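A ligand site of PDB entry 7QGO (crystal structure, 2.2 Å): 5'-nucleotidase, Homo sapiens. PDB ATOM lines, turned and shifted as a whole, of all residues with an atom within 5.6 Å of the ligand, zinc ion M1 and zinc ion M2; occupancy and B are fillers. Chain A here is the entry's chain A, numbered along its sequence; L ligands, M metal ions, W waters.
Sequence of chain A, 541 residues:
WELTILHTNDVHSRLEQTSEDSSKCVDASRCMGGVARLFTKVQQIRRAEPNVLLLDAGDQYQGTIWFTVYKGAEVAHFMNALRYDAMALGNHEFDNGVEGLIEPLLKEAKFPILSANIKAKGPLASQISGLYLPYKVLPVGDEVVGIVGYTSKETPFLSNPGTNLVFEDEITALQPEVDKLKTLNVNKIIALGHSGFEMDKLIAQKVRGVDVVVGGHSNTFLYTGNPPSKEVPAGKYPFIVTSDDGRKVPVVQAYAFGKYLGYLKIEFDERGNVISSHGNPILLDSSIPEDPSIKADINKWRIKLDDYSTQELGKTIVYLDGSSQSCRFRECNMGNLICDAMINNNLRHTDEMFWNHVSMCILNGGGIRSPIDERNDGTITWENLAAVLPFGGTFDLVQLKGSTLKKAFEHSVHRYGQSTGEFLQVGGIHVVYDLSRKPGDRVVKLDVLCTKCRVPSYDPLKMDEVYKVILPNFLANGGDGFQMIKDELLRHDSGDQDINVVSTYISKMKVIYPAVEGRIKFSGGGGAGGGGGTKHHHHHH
The side-chain carboxylate of Asp 480 lies within hydrogen-bond range of an oxygen (O9) of the ligand (2.6 Å). The guanidinium group (NH1) of Arg 369 lies within salt-bridge range of an oxygen (O5) of the ligand, 2.6 Å away. ND2 of Asn 364 sits at hydrogen-bond distance from O10 of the ligand (2.8 Å). The guanidinium group of Arg 328 is in salt-bridge range of an oxygen (O1) of the ligand (3.1 Å). O of Gly 421 sits at hydrogen-bond distance from O9 of the ligand (3.3 Å). O5 of the ligand lies within hydrogen-bond range of NE2 of His 92, at 2.7 Å. An oxygen (O12) of the ligand lies close to the side-chain amide oxygen (OE1) of Gln 62.
The backbone NH (N) of Gly 367 lies close to the side-chain amide nitrogen (ND2) of Asn 364 (3.1 Å). The guanidinium group (NH1) of Arg 328 lies within hydrogen-bond range of the backbone carbonyl oxygen (O) of Ser 419 (2.9 Å). A ring nitrogen (ND1) of His 92 is in hydrogen-bond range of the side-chain carboxylate of Asp 95 (2.4 Å). The guanidinium group (NH1) of Arg 369 sits at hydrogen-bond distance from a ring nitrogen (NE2) of His 92, at 3.4 Å. O of Gly 421 sits at hydrogen-bond distance from N of Gly 365, at 3.5 Å. The backbone NH (N) of Gly 366 is in hydrogen-bond range of the backbone carbonyl oxygen (O) of Gly 421 (3.1 Å). The side-chain carboxylate (OD2) of Asp 10 lies close to the side-chain amide oxygen (OD1) of Asn 219. The backbone carbonyl oxygen of Gln 62 lies within hydrogen-bond range of a ring nitrogen (ND1) of His 12.
The backbone carbonyl oxygen (O) of Leu 158 sits close to an oxygen (O11) of the ligand (3.1 Å). O of Phe 391 lies close to O13 of the ligand (3.3 Å). CB of Asp 95 touches O12 of the ligand, 3.3 Å away. CA of Ser 159 touches C19 of the ligand (3.9999 Å). ND2 of Asn 160 touches C17 of the ligand (3.5 Å). Gly 366 touches the ligand. Gly 367 touches the ligand (CA to O10, 3.4 Å). Phe 474 touches the ligand (CE1 to C5, 3.5 Å). Hydrophobic or aromatic side chains that line the ligand: His 12, His 92, His 217, Phe 391 and Phe 474. Within 4 Å of the ligand: Asp 10, His 12, Asp 59, Gln 62, Asn 91, His 92, Asp 95, Leu 158, Ser 159, Asn 160, His 217, Arg 328, Asn 364, Gly 366, Gly 367, Arg 369, Phe 391, Gly 421, Phe 474 and Asp 480. The nearest printed residue that does not touch the ligand is Pro 390 (4.04 Å).
Merely in contact with zinc ion M1: Asn 219 (3.9 Å). Along chain A the residues within 4 Å of zinc ion M1 span positions 10 to 219.
Five residues have an atom within 4 Å of zinc ion M2: Asp 10, Asp 59, Asn 91, His 194 and His 217.
Zinc ion M1 is bound by O4 of the ligand, 2.0 Å away. NE2 of His 12 binds zinc ion M1, at 2.0 Å. OD1 of Asp 10 is bound to zinc ion M1 (2.3 Å). Zinc ion M1 is bound by OD2 of Asp 59 (2.4 Å).
OD1 of Asn 91 is bound to zinc ion M2 (2.1 Å). Zinc ion M2 is bound by NE2 of His 194 (2.1 Å). Zinc ion M2 is bound by ND1 of His 217 (2.1 Å). O3 of the ligand is bound to zinc ion M2. OD2 of Asp 59 binds zinc ion M2 (2.3 Å).
Water W1 lies within hydrogen-bond range of the side-chain amide oxygen (OD1) of Asn 364 and an oxygen (O10) of the ligand.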
ATOM      1  N   ASP A  10      -1.825 -35.066  10.315  1.00  0.00           N
ATOM      2  CA  ASP A  10      -2.809 -34.005  10.506  1.00  0.00           C
ATOM      3  C   ASP A  10      -3.077 -33.665  11.967  1.00  0.00           C
ATOM      4  O   ASP A  10      -4.223 -33.496  12.362  1.00  0.00           O
ATOM      5  CB  ASP A  10      -4.101 -34.372   9.765  1.00  0.00           C
ATOM      6  CG  ASP A  10      -3.816 -34.739   8.322  1.00  0.00           C
ATOM      7  OD1 ASP A  10      -3.511 -33.839   7.529  1.00  0.00           O
ATOM      8  OD2 ASP A  10      -3.877 -35.932   7.985  1.00  0.00           O
ATOM      9  N   HIS A  12      -2.429 -30.888  13.380  1.00  0.00           N
ATOM     10  CA  HIS A  12      -3.009 -29.557  13.288  1.00  0.00           C
ATOM     11  C   HIS A  12      -2.955 -28.759  14.594  1.00  0.00           C
ATOM     12  O   HIS A  12      -3.994 -28.365  15.142  1.00  0.00           O
ATOM     13  CB  HIS A  12      -4.437 -29.572  12.695  1.00  0.00           C
ATOM     14  CG  HIS A  12      -4.429 -29.861  11.231  1.00  0.00           C
ATOM     15  ND1 HIS A  12      -3.590 -29.172  10.349  1.00  0.00           N
ATOM     16  CD2 HIS A  12      -5.115 -30.803  10.528  1.00  0.00           C
ATOM     17  CE1 HIS A  12      -3.813 -29.683   9.157  1.00  0.00           C
ATOM     18  NE2 HIS A  12      -4.729 -30.668   9.202  1.00  0.00           N
ATOM     19  N   ASP A  59       1.185 -32.007   8.122  1.00  0.00           N
ATOM     20  CA  ASP A  59       0.142 -31.132   8.626  1.00  0.00           C
ATOM     21  C   ASP A  59       0.140 -31.001  10.123  1.00  0.00           C
ATOM     22  O   ASP A  59      -0.896 -31.117  10.771  1.00  0.00           O
ATOM     23  CB  ASP A  59      -1.234 -31.528   8.073  1.00  0.00           C
ATOM     24  CG  ASP A  59      -1.586 -30.910   6.740  1.00  0.00           C
ATOM     25  OD1 ASP A  59      -0.692 -30.313   6.097  1.00  0.00           O
ATOM     26  OD2 ASP A  59      -2.764 -31.027   6.321  1.00  0.00           O
ATOM     27  N   GLN A  62      -0.765 -25.294  11.446  1.00  0.00           N
ATOM     28  CA  GLN A  62      -2.138 -24.786  11.340  1.00  0.00           C
ATOM     29  C   GLN A  62      -3.181 -25.555  12.134  1.00  0.00           C
ATOM     30  O   GLN A  62      -3.283 -26.758  11.942  1.00  0.00           O
ATOM     31  CB  GLN A  62      -2.558 -24.729   9.863  1.00  0.00           C
ATOM     32  CG  GLN A  62      -4.049 -24.428   9.608  1.00  0.00           C
ATOM     33  CD  GLN A  62      -4.252 -23.015   9.240  1.00  0.00           C
ATOM     34  OE1 GLN A  62      -3.517 -22.097   9.667  1.00  0.00           O
ATOM     35  NE2 GLN A  62      -5.253 -22.793   8.405  1.00  0.00           N
ATOM     36  N   PHE A  67      -0.177 -22.330  16.823  1.00  0.00           N
ATOM     37  CA  PHE A  67       0.407 -22.006  15.540  1.00  0.00           C
ATOM     38  C   PHE A  67       0.347 -20.492  15.268  1.00  0.00           C
ATOM     39  O   PHE A  67       1.318 -19.910  14.780  1.00  0.00           O
ATOM     40  CB  PHE A  67      -0.305 -22.767  14.438  1.00  0.00           C
ATOM     41  CG  PHE A  67       0.437 -22.601  13.146  1.00  0.00           C
ATOM     42  CD1 PHE A  67       1.721 -23.081  13.015  1.00  0.00           C
ATOM     43  CD2 PHE A  67      -0.109 -21.882  12.099  1.00  0.00           C
ATOM     44  CE1 PHE A  67       2.447 -22.858  11.849  1.00  0.00           C
ATOM     45  CE2 PHE A  67       0.591 -21.696  10.929  1.00  0.00           C
ATOM     46  CZ  PHE A  67       1.868 -22.184  10.815  1.00  0.00           C
ATOM     47  N   GLY A  90       3.613 -31.734   4.731  1.00  0.00           N
ATOM     48  CA  GLY A  90       2.216 -31.637   4.358  1.00  0.00           C
ATOM     49  C   GLY A  90       1.912 -30.321   3.663  1.00  0.00           C
ATOM     50  O   GLY A  90       2.796 -29.452   3.573  1.00  0.00           O
ATOM     51  N   ASN A  91       0.679 -30.149   3.158  1.00  0.00           N
ATOM     52  CA  ASN A  91       0.349 -28.904   2.467  1.00  0.00           C
ATOM     53  C   ASN A  91       0.372 -27.689   3.426  1.00  0.00           C
ATOM     54  O   ASN A  91       0.987 -26.666   3.095  1.00  0.00           O
ATOM     55  CB  ASN A  91      -0.930 -28.989   1.665  1.00  0.00           C
ATOM     56  CG  ASN A  91      -2.105 -29.276   2.493  1.00  0.00           C
ATOM     57  OD1 ASN A  91      -2.236 -30.367   3.041  1.00  0.00           O
ATOM     58  ND2 ASN A  91      -2.991 -28.290   2.618  1.00  0.00           N
ATOM     59  N   HIS A  92      -0.102 -27.886   4.650  1.00  0.00           N
ATOM     60  CA  HIS A  92      -0.127 -26.864   5.698  1.00  0.00           C
ATOM     61  C   HIS A  92       1.236 -26.370   6.210  1.00  0.00           C
ATOM     62  O   HIS A  92       1.272 -25.306   6.830  1.00  0.00           O
ATOM     63  CB  HIS A  92      -0.990 -27.306   6.879  1.00  0.00           C
ATOM     64  CG  HIS A  92      -2.462 -27.181   6.630  1.00  0.00           C
ATOM     65  ND1 HIS A  92      -3.107 -25.957   6.698  1.00  0.00           N
ATOM     66  CD2 HIS A  92      -3.364 -28.132   6.283  1.00  0.00           C
ATOM     67  CE1 HIS A  92      -4.379 -26.204   6.437  1.00  0.00           C
ATOM     68  NE2 HIS A  92      -4.589 -27.492   6.171  1.00  0.00           N
ATOM     69  N   ASP A  95       1.793 -22.815   4.875  1.00  0.00           N
ATOM     70  CA  ASP A  95       0.780 -21.804   5.137  1.00  0.00           C
ATOM     71  C   ASP A  95       1.391 -20.424   5.449  1.00  0.00           C
ATOM     72  O   ASP A  95       0.769 -19.405   5.143  1.00  0.00           O
ATOM     73  CB  ASP A  95      -0.201 -22.260   6.237  1.00  0.00           C
ATOM     74  CG  ASP A  95      -1.145 -23.376   5.805  1.00  0.00           C
ATOM     75  OD1 ASP A  95      -1.187 -23.708   4.609  1.00  0.00           O
ATOM     76  OD2 ASP A  95      -1.845 -23.910   6.678  1.00  0.00           O
ATOM     77  N   ASN A  96       2.592 -20.381   6.020  1.00  0.00           N
ATOM     78  CA  ASN A  96       3.286 -19.115   6.254  1.00  0.00           C
ATOM     79  C   ASN A  96       4.399 -18.898   5.200  1.00  0.00           C
ATOM     80  O   ASN A  96       5.401 -18.254   5.502  1.00  0.00           O
ATOM     81  CB  ASN A  96       3.906 -19.059   7.667  1.00  0.00           C
ATOM     82  CG  ASN A  96       2.934 -19.128   8.814  1.00  0.00           C
ATOM     83  OD1 ASN A  96       1.716 -19.245   8.616  1.00  0.00           O
ATOM     84  ND2 ASN A  96       3.452 -19.059  10.037  1.00  0.00           N
ATOM     85  N   PHE A 157      -2.604 -24.961  -4.539  1.00  0.00           N
ATOM     86  CA  PHE A 157      -4.027 -24.688  -4.613  1.00  0.00           C
ATOM     87  C   PHE A 157      -4.725 -24.718  -3.237  1.00  0.00           C
ATOM     88  O   PHE A 157      -5.932 -24.493  -3.161  1.00  0.00           O
ATOM     89  CB  PHE A 157      -4.707 -25.679  -5.575  1.00  0.00           C
ATOM     90  CG  PHE A 157      -4.051 -25.720  -6.932  1.00  0.00           C
ATOM     91  CD1 PHE A 157      -4.288 -24.724  -7.870  1.00  0.00           C
ATOM     92  CD2 PHE A 157      -3.153 -26.724  -7.250  1.00  0.00           C
ATOM     93  CE1 PHE A 157      -3.650 -24.745  -9.106  1.00  0.00           C
ATOM     94  CE2 PHE A 157      -2.514 -26.743  -8.473  1.00  0.00           C
ATOM     95  CZ  PHE A 157      -2.767 -25.751  -9.408  1.00  0.00           C
ATOM     96  N   LEU A 158      -3.948 -24.986  -2.163  1.00  0.00           N
ATOM     97  CA  LEU A 158      -4.419 -25.064  -0.797  1.00  0.00           C
ATOM     98  C   LEU A 158      -3.523 -24.300   0.193  1.00  0.00           C
ATOM     99  O   LEU A 158      -3.881 -24.242   1.375  1.00  0.00           O
ATOM    100  CB  LEU A 158      -4.442 -26.542  -0.365  1.00  0.00           C
ATOM    101  CG  LEU A 158      -5.300 -27.473  -1.171  1.00  0.00           C
ATOM    102  CD1 LEU A 158      -4.715 -28.857  -1.162  1.00  0.00           C
ATOM    103  CD2 LEU A 158      -6.720 -27.481  -0.655  1.00  0.00           C
ATOM    104  N   SER A 159      -2.371 -23.756  -0.237  1.00  0.00           N
ATOM    105  CA  SER A 159      -1.428 -23.153   0.696  1.00  0.00           C
ATOM    106  C   SER A 159      -0.587 -21.999   0.084  1.00  0.00           C
ATOM    107  O   SER A 159      -0.951 -21.473  -0.967  1.00  0.00           O
ATOM    108  CB  SER A 159      -0.531 -24.266   1.250  1.00  0.00           C
ATOM    109  OG  SER A 159       0.209 -23.852   2.387  1.00  0.00           O
ATOM    110  N   ASN A 160       0.530 -21.608   0.727  1.00  0.00           N
ATOM    111  CA  ASN A 160       1.372 -20.545   0.215  1.00  0.00           C
ATOM    112  C   ASN A 160       2.817 -21.026  -0.097  1.00  0.00           C
ATOM    113  O   ASN A 160       3.770 -20.432   0.408  1.00  0.00           O
ATOM    114  CB  ASN A 160       1.368 -19.351   1.188  1.00  0.00           C
ATOM    115  CG  ASN A 160      -0.023 -18.862   1.515  1.00  0.00           C
ATOM    116  OD1 ASN A 160      -0.615 -18.077   0.778  1.00  0.00           O
ATOM    117  ND2 ASN A 160      -0.583 -19.337   2.618  1.00  0.00           N
ATOM    118  N   HIS A 194       1.956 -37.043   2.358  1.00  0.00           N
ATOM    119  CA  HIS A 194       0.754 -36.289   2.619  1.00  0.00           C
ATOM    120  C   HIS A 194      -0.062 -35.988   1.366  1.00  0.00           C
ATOM    121  O   HIS A 194      -0.024 -34.868   0.864  1.00  0.00           O
ATOM    122  CB  HIS A 194       1.184 -35.003   3.308  1.00  0.00           C
ATOM    123  CG  HIS A 194       0.040 -34.304   3.946  1.00  0.00           C
ATOM    124  ND1 HIS A 194      -0.463 -34.708   5.166  1.00  0.00           N
ATOM    125  CD2 HIS A 194      -0.702 -33.276   3.476  1.00  0.00           C
ATOM    126  CE1 HIS A 194      -1.479 -33.904   5.421  1.00  0.00           C
ATOM    127  NE2 HIS A 194      -1.667 -33.032   4.433  1.00  0.00           N
ATOM    128  N   HIS A 217      -3.528 -36.334   5.165  1.00  0.00           N
ATOM    129  CA  HIS A 217      -4.269 -35.355   4.328  1.00  0.00           C
ATOM    130  C   HIS A 217      -5.777 -35.571   4.220  1.00  0.00           C
ATOM    131  O   HIS A 217      -6.516 -34.592   4.297  1.00  0.00           O
ATOM    132  CB  HIS A 217      -3.693 -35.255   2.934  1.00  0.00           C
ATOM    133  CG  HIS A 217      -4.215 -34.092   2.146  1.00  0.00           C
ATOM    134  ND1 HIS A 217      -3.938 -32.789   2.519  1.00  0.00           N
ATOM    135  CD2 HIS A 217      -4.936 -34.075   1.011  1.00  0.00           C
ATOM    136  CE1 HIS A 217      -4.520 -32.039   1.615  1.00  0.00           C
ATOM    137  NE2 HIS A 217      -5.138 -32.758   0.691  1.00  0.00           N
ATOM    138  N   ASN A 219      -7.521 -37.368   6.422  1.00  0.00           N
ATOM    139  CA  ASN A 219      -7.946 -37.600   7.816  1.00  0.00           C
ATOM    140  C   ASN A 219      -8.635 -38.942   7.975  1.00  0.00           C
ATOM    141  O   ASN A 219      -9.561 -39.083   8.764  1.00  0.00           O
ATOM    142  CB  ASN A 219      -8.836 -36.469   8.317  1.00  0.00           C
ATOM    143  CG  ASN A 219      -8.134 -35.167   8.630  1.00  0.00           C
ATOM    144  OD1 ASN A 219      -7.033 -34.862   8.183  1.00  0.00           O
ATOM    145  ND2 ASN A 219      -8.810 -34.327   9.413  1.00  0.00           N
ATOM    146  N   ARG A 328     -19.464 -30.787   6.029  1.00  0.00           N
ATOM    147  CA  ARG A 328     -19.175 -31.144   4.627  1.00  0.00           C
ATOM    148  C   ARG A 328     -20.242 -32.088   4.024  1.00  0.00           C
ATOM    149  O   ARG A 328     -20.103 -32.493   2.857  1.00  0.00           O
ATOM    150  CB  ARG A 328     -17.779 -31.729   4.458  1.00  0.00           C
ATOM    151  CG  ARG A 328     -16.702 -30.945   5.202  1.00  0.00           C
ATOM    152  CD  ARG A 328     -15.331 -31.508   4.914  1.00  0.00           C
ATOM    153  NE  ARG A 328     -14.283 -30.704   5.549  1.00  0.00           N
ATOM    154  CZ  ARG A 328     -12.991 -30.785   5.245  1.00  0.00           C
ATOM    155  NH1 ARG A 328     -12.565 -31.624   4.311  1.00  0.00           N
ATOM    156  NH2 ARG A 328     -12.107 -30.019   5.888  1.00  0.00           N
ATOM    157  N   ASN A 364     -17.493 -22.182   2.158  1.00  0.00           N
ATOM    158  CA  ASN A 364     -16.975 -23.523   1.946  1.00  0.00           C
ATOM    159  C   ASN A 364     -16.866 -24.200   3.292  1.00  0.00           C
ATOM    160  O   ASN A 364     -16.238 -23.623   4.186  1.00  0.00           O
ATOM    161  CB  ASN A 364     -15.631 -23.456   1.178  1.00  0.00           C
ATOM    162  CG  ASN A 364     -14.452 -22.776   1.856  1.00  0.00           C
ATOM    163  OD1 ASN A 364     -14.354 -21.551   1.986  1.00  0.00           O
ATOM    164  ND2 ASN A 364     -13.490 -23.578   2.266  1.00  0.00           N
ATOM    165  N   GLY A 365     -17.596 -25.307   3.499  1.00  0.00           N
ATOM    166  CA  GLY A 365     -17.616 -26.066   4.750  1.00  0.00           C
ATOM    167  C   GLY A 365     -16.237 -26.551   5.214  1.00  0.00           C
ATOM    168  O   GLY A 365     -15.986 -26.695   6.412  1.00  0.00           O
ATOM    169  N   GLY A 366     -15.322 -26.761   4.276  1.00  0.00           N
ATOM    170  CA  GLY A 366     -13.943 -27.106   4.594  1.00  0.00           C
ATOM    171  C   GLY A 366     -13.178 -25.945   5.222  1.00  0.00           C
ATOM    172  O   GLY A 366     -12.098 -26.151   5.777  1.00  0.00           O
ATOM    173  N   GLY A 367     -13.721 -24.732   5.137  1.00  0.00           N
ATOM    174  CA  GLY A 367     -13.143 -23.553   5.778  1.00  0.00           C
ATOM    175  C   GLY A 367     -13.443 -23.489   7.271  1.00  0.00           C
ATOM    176  O   GLY A 367     -12.847 -22.684   7.990  1.00  0.00           O
ATOM    177  N   ARG A 369     -13.054 -25.286  10.521  1.00  0.00           N
ATOM    178  CA  ARG A 369     -12.045 -26.279  10.930  1.00  0.00           C
ATOM    179  C   ARG A 369     -12.232 -26.915  12.301  1.00  0.00           C
ATOM    180  O   ARG A 369     -11.485 -27.830  12.638  1.00  0.00           O
ATOM    181  CB  ARG A 369     -10.658 -25.637  10.835  1.00  0.00           C
ATOM    182  CG  ARG A 369     -10.415 -24.920   9.514  1.00  0.00           C
ATOM    183  CD  ARG A 369     -10.295 -25.874   8.348  1.00  0.00           C
ATOM    184  NE  ARG A 369      -9.078 -26.683   8.388  1.00  0.00           N
ATOM    185  CZ  ARG A 369      -8.739 -27.571   7.464  1.00  0.00           C
ATOM    186  NH1 ARG A 369      -7.625 -28.277   7.593  1.00  0.00           N
ATOM    187  NH2 ARG A 369      -9.507 -27.762   6.399  1.00  0.00           N
ATOM    188  N   PRO A 390      -8.809 -20.624  11.119  1.00  0.00           N
ATOM    189  CA  PRO A 390      -7.369 -20.386  11.185  1.00  0.00           C
ATOM    190  C   PRO A 390      -6.694 -19.786   9.930  1.00  0.00           C
ATOM    191  O   PRO A 390      -5.538 -19.406  10.027  1.00  0.00           O
ATOM    192  CB  PRO A 390      -6.822 -21.778  11.482  1.00  0.00           C
ATOM    193  CG  PRO A 390      -7.759 -22.691  10.759  1.00  0.00           C
ATOM    194  CD  PRO A 390      -9.106 -22.023  10.739  1.00  0.00           C
ATOM    195  N   PHE A 391      -7.382 -19.724   8.782  1.00  0.00           N
ATOM    196  CA  PHE A 391      -6.766 -19.201   7.548  1.00  0.00           C
ATOM    197  C   PHE A 391      -6.574 -17.679   7.505  1.00  0.00           C
ATOM    198  O   PHE A 391      -5.876 -17.182   6.625  1.00  0.00           O
ATOM    199  CB  PHE A 391      -7.553 -19.653   6.314  1.00  0.00           C
ATOM    200  CG  PHE A 391      -7.686 -21.145   6.172  1.00  0.00           C
ATOM    201  CD1 PHE A 391      -6.739 -21.879   5.494  1.00  0.00           C
ATOM    202  CD2 PHE A 391      -8.800 -21.802   6.659  1.00  0.00           C
ATOM    203  CE1 PHE A 391      -6.877 -23.244   5.339  1.00  0.00           C
ATOM    204  CE2 PHE A 391      -8.947 -23.164   6.490  1.00  0.00           C
ATOM    205  CZ  PHE A 391      -7.977 -23.883   5.829  1.00  0.00           C
ATOM    206  N   GLY A 392      -7.232 -16.955   8.405  1.00  0.00           N
ATOM    207  CA  GLY A 392      -7.109 -15.515   8.495  1.00  0.00           C
ATOM    208  C   GLY A 392      -7.505 -14.727   7.260  1.00  0.00           C
ATOM    209  O   GLY A 392      -6.967 -13.648   7.019  1.00  0.00           O
ATOM    210  N   SER A 419     -16.194 -36.358   2.074  1.00  0.00           N
ATOM    211  CA  SER A 419     -15.691 -35.399   3.088  1.00  0.00           C
ATOM    212  C   SER A 419     -14.974 -34.201   2.398  1.00  0.00           C
ATOM    213  O   SER A 419     -13.969 -33.674   2.870  1.00  0.00           O
ATOM    214  CB  SER A 419     -14.782 -36.084   4.101  1.00  0.00           C
ATOM    215  OG  SER A 419     -14.693 -35.332   5.305  1.00  0.00           O
ATOM    216  N   THR A 420     -15.526 -33.818   1.271  1.00  0.00           N
ATOM    217  CA  THR A 420     -15.022 -32.774   0.394  1.00  0.00           C
ATOM    218  C   THR A 420     -15.456 -31.393   0.910  1.00  0.00           C
ATOM    219  O   THR A 420     -16.646 -31.161   1.186  1.00  0.00           O
ATOM    220  CB  THR A 420     -15.401 -33.130  -1.049  1.00  0.00           C
ATOM    221  OG1 THR A 420     -16.732 -33.675  -1.110  1.00  0.00           O
ATOM    222  CG2 THR A 420     -14.483 -34.162  -1.609  1.00  0.00           C
ATOM    223  N   GLY A 421     -14.461 -30.519   1.070  1.00  0.00           N
ATOM    224  CA  GLY A 421     -14.599 -29.174   1.609  1.00  0.00           C
ATOM    225  C   GLY A 421     -15.382 -28.185   0.759  1.00  0.00           C
ATOM    226  O   GLY A 421     -15.665 -27.075   1.231  1.00  0.00           O
ATOM    227  N   GLU A 422     -15.736 -28.573  -0.476  1.00  0.00           N
ATOM    228  CA  GLU A 422     -16.459 -27.674  -1.356  1.00  0.00           C
ATOM    229  C   GLU A 422     -17.971 -27.608  -1.081  1.00  0.00           C
ATOM    230  O   GLU A 422     -18.640 -26.801  -1.721  1.00  0.00           O
ATOM    231  CB  GLU A 422     -16.146 -27.956  -2.841  1.00  0.00           C
ATOM    232  CG  GLU A 422     -17.030 -28.996  -3.520  1.00  0.00           C
ATOM    233  CD  GLU A 422     -16.486 -30.402  -3.539  1.00  0.00           C
ATOM    234  OE1 GLU A 422     -17.205 -31.303  -4.023  1.00  0.00           O
ATOM    235  OE2 GLU A 422     -15.339 -30.612  -3.077  1.00  0.00           O
ATOM    236  N   PHE A 474     -11.328 -16.763  -0.379  1.00  0.00           N
ATOM    237  CA  PHE A 474     -10.894 -18.044  -0.894  1.00  0.00           C
ATOM    238  C   PHE A 474     -11.828 -18.501  -2.026  1.00  0.00           C
ATOM    239  O   PHE A 474     -11.340 -18.862  -3.096  1.00  0.00           O
ATOM    240  CB  PHE A 474     -10.869 -19.089   0.240  1.00  0.00           C
ATOM    241  CG  PHE A 474     -10.604 -20.509  -0.223  1.00  0.00           C
ATOM    242  CD1 PHE A 474      -9.367 -20.869  -0.730  1.00  0.00           C
ATOM    243  CD2 PHE A 474     -11.574 -21.493  -0.093  1.00  0.00           C
ATOM    244  CE1 PHE A 474      -9.122 -22.176  -1.135  1.00  0.00           C
ATOM    245  CE2 PHE A 474     -11.322 -22.792  -0.515  1.00  0.00           C
ATOM    246  CZ  PHE A 474     -10.105 -23.126  -1.019  1.00  0.00           C
ATOM    247  N   ASP A 480     -11.117 -24.239  -4.145  1.00  0.00           N
ATOM    248  CA  ASP A 480     -11.956 -25.438  -4.076  1.00  0.00           C
ATOM    249  C   ASP A 480     -12.594 -25.816  -5.425  1.00  0.00           C
ATOM    250  O   ASP A 480     -13.595 -26.532  -5.429  1.00  0.00           O
ATOM    251  CB  ASP A 480     -13.059 -25.302  -3.003  1.00  0.00           C
ATOM    252  CG  ASP A 480     -12.825 -26.140  -1.765  1.00  0.00           C
ATOM    253  OD1 ASP A 480     -12.031 -27.094  -1.830  1.00  0.00           O
ATOM    254  OD2 ASP A 480     -13.454 -25.838  -0.734  1.00  0.00           O
HETATM  255  N1  LIG L   1      -8.890 -22.202   2.601  1.00  0.00           N
HETATM  256  C1  LIG L   1      -9.833 -23.209   2.813  1.00  0.00           C
HETATM  257  C2  LIG L   1      -9.270 -20.856   3.039  1.00  0.00           C
HETATM  258  C3  LIG L   1      -8.246 -24.739   1.833  1.00  0.00           C
HETATM  259  C4  LIG L   1      -7.338 -23.764   1.601  1.00  0.00           C
HETATM  260  C5  LIG L   1      -7.657 -22.440   1.995  1.00  0.00           C
HETATM  261  C6  LIG L   1      -4.278 -20.346   2.471  1.00  0.00           C
HETATM  262  C7  LIG L   1      -3.314 -19.821   5.058  1.00  0.00           C
HETATM  263  C8  LIG L   1      -4.169 -19.043   2.939  1.00  0.00           C
HETATM  264  C9  LIG L   1      -2.211 -17.877   7.993  1.00  0.00           C
HETATM  265  O1  LIG L   1      -9.337 -31.398   5.617  1.00  0.00           O
HETATM  266  P1  LIG L   1      -8.870 -31.056   4.246  1.00  0.00           P
HETATM  267  O2  LIG L   1      -9.646 -31.899   3.197  1.00  0.00           O
HETATM  268  C10 LIG L   1      -7.133 -31.268   3.829  1.00  0.00           C
HETATM  269  P2  LIG L   1      -5.987 -30.333   4.840  1.00  0.00           P
HETATM  270  O3  LIG L   1      -4.696 -30.046   4.132  1.00  0.00           O
HETATM  271  O4  LIG L   1      -5.801 -31.183   6.100  1.00  0.00           O
HETATM  272  O5  LIG L   1      -6.673 -29.031   5.272  1.00  0.00           O
HETATM  273  O6  LIG L   1      -9.007 -29.515   3.932  1.00  0.00           O
HETATM  274  C11 LIG L   1      -9.034 -28.925   2.626  1.00  0.00           C
HETATM  275  C12 LIG L   1     -10.113 -27.880   2.568  1.00  0.00           C
HETATM  276  C13 LIG L   1     -10.447 -27.395   1.167  1.00  0.00           C
HETATM  277  O7  LIG L   1     -11.282 -28.350   0.502  1.00  0.00           O
HETATM  278  O8  LIG L   1      -9.703 -26.673   3.247  1.00  0.00           O
HETATM  279  C14 LIG L   1     -10.411 -25.572   2.707  1.00  0.00           C
HETATM  280  C15 LIG L   1     -11.144 -26.071   1.450  1.00  0.00           C
HETATM  281  O9  LIG L   1     -12.538 -26.286   1.687  1.00  0.00           O
HETATM  282  N2  LIG L   1      -9.462 -24.478   2.432  1.00  0.00           N
HETATM  283  O10 LIG L   1     -10.934 -22.941   3.263  1.00  0.00           O
HETATM  284  N3  LIG L   1      -6.900 -21.415   1.796  1.00  0.00           N
HETATM  285  O11 LIG L   1      -5.689 -21.771   1.138  1.00  0.00           O
HETATM  286  C16 LIG L   1      -4.832 -20.628   1.108  1.00  0.00           C
HETATM  287  C17 LIG L   1      -3.697 -18.779   4.211  1.00  0.00           C
HETATM  288  C18 LIG L   1      -3.423 -21.124   4.590  1.00  0.00           C
HETATM  289  C19 LIG L   1      -3.879 -21.383   3.315  1.00  0.00           C
HETATM  290  C20 LIG L   1      -2.893 -19.547   6.457  1.00  0.00           C
HETATM  291  O12 LIG L   1      -2.725 -20.392   7.296  1.00  0.00           O
HETATM  292  O13 LIG L   1      -2.778 -18.238   6.705  1.00  0.00           O
HETATM  293 ZN    ZN M   1      -4.692 -31.826   7.572  1.00  0.00          ZN
HETATM  294 ZN    ZN M   2      -3.278 -31.692   4.222  1.00  0.00          ZN
HETATM  295  O   HOH W   1     -12.808 -20.172   3.970  1.00  0.00           O
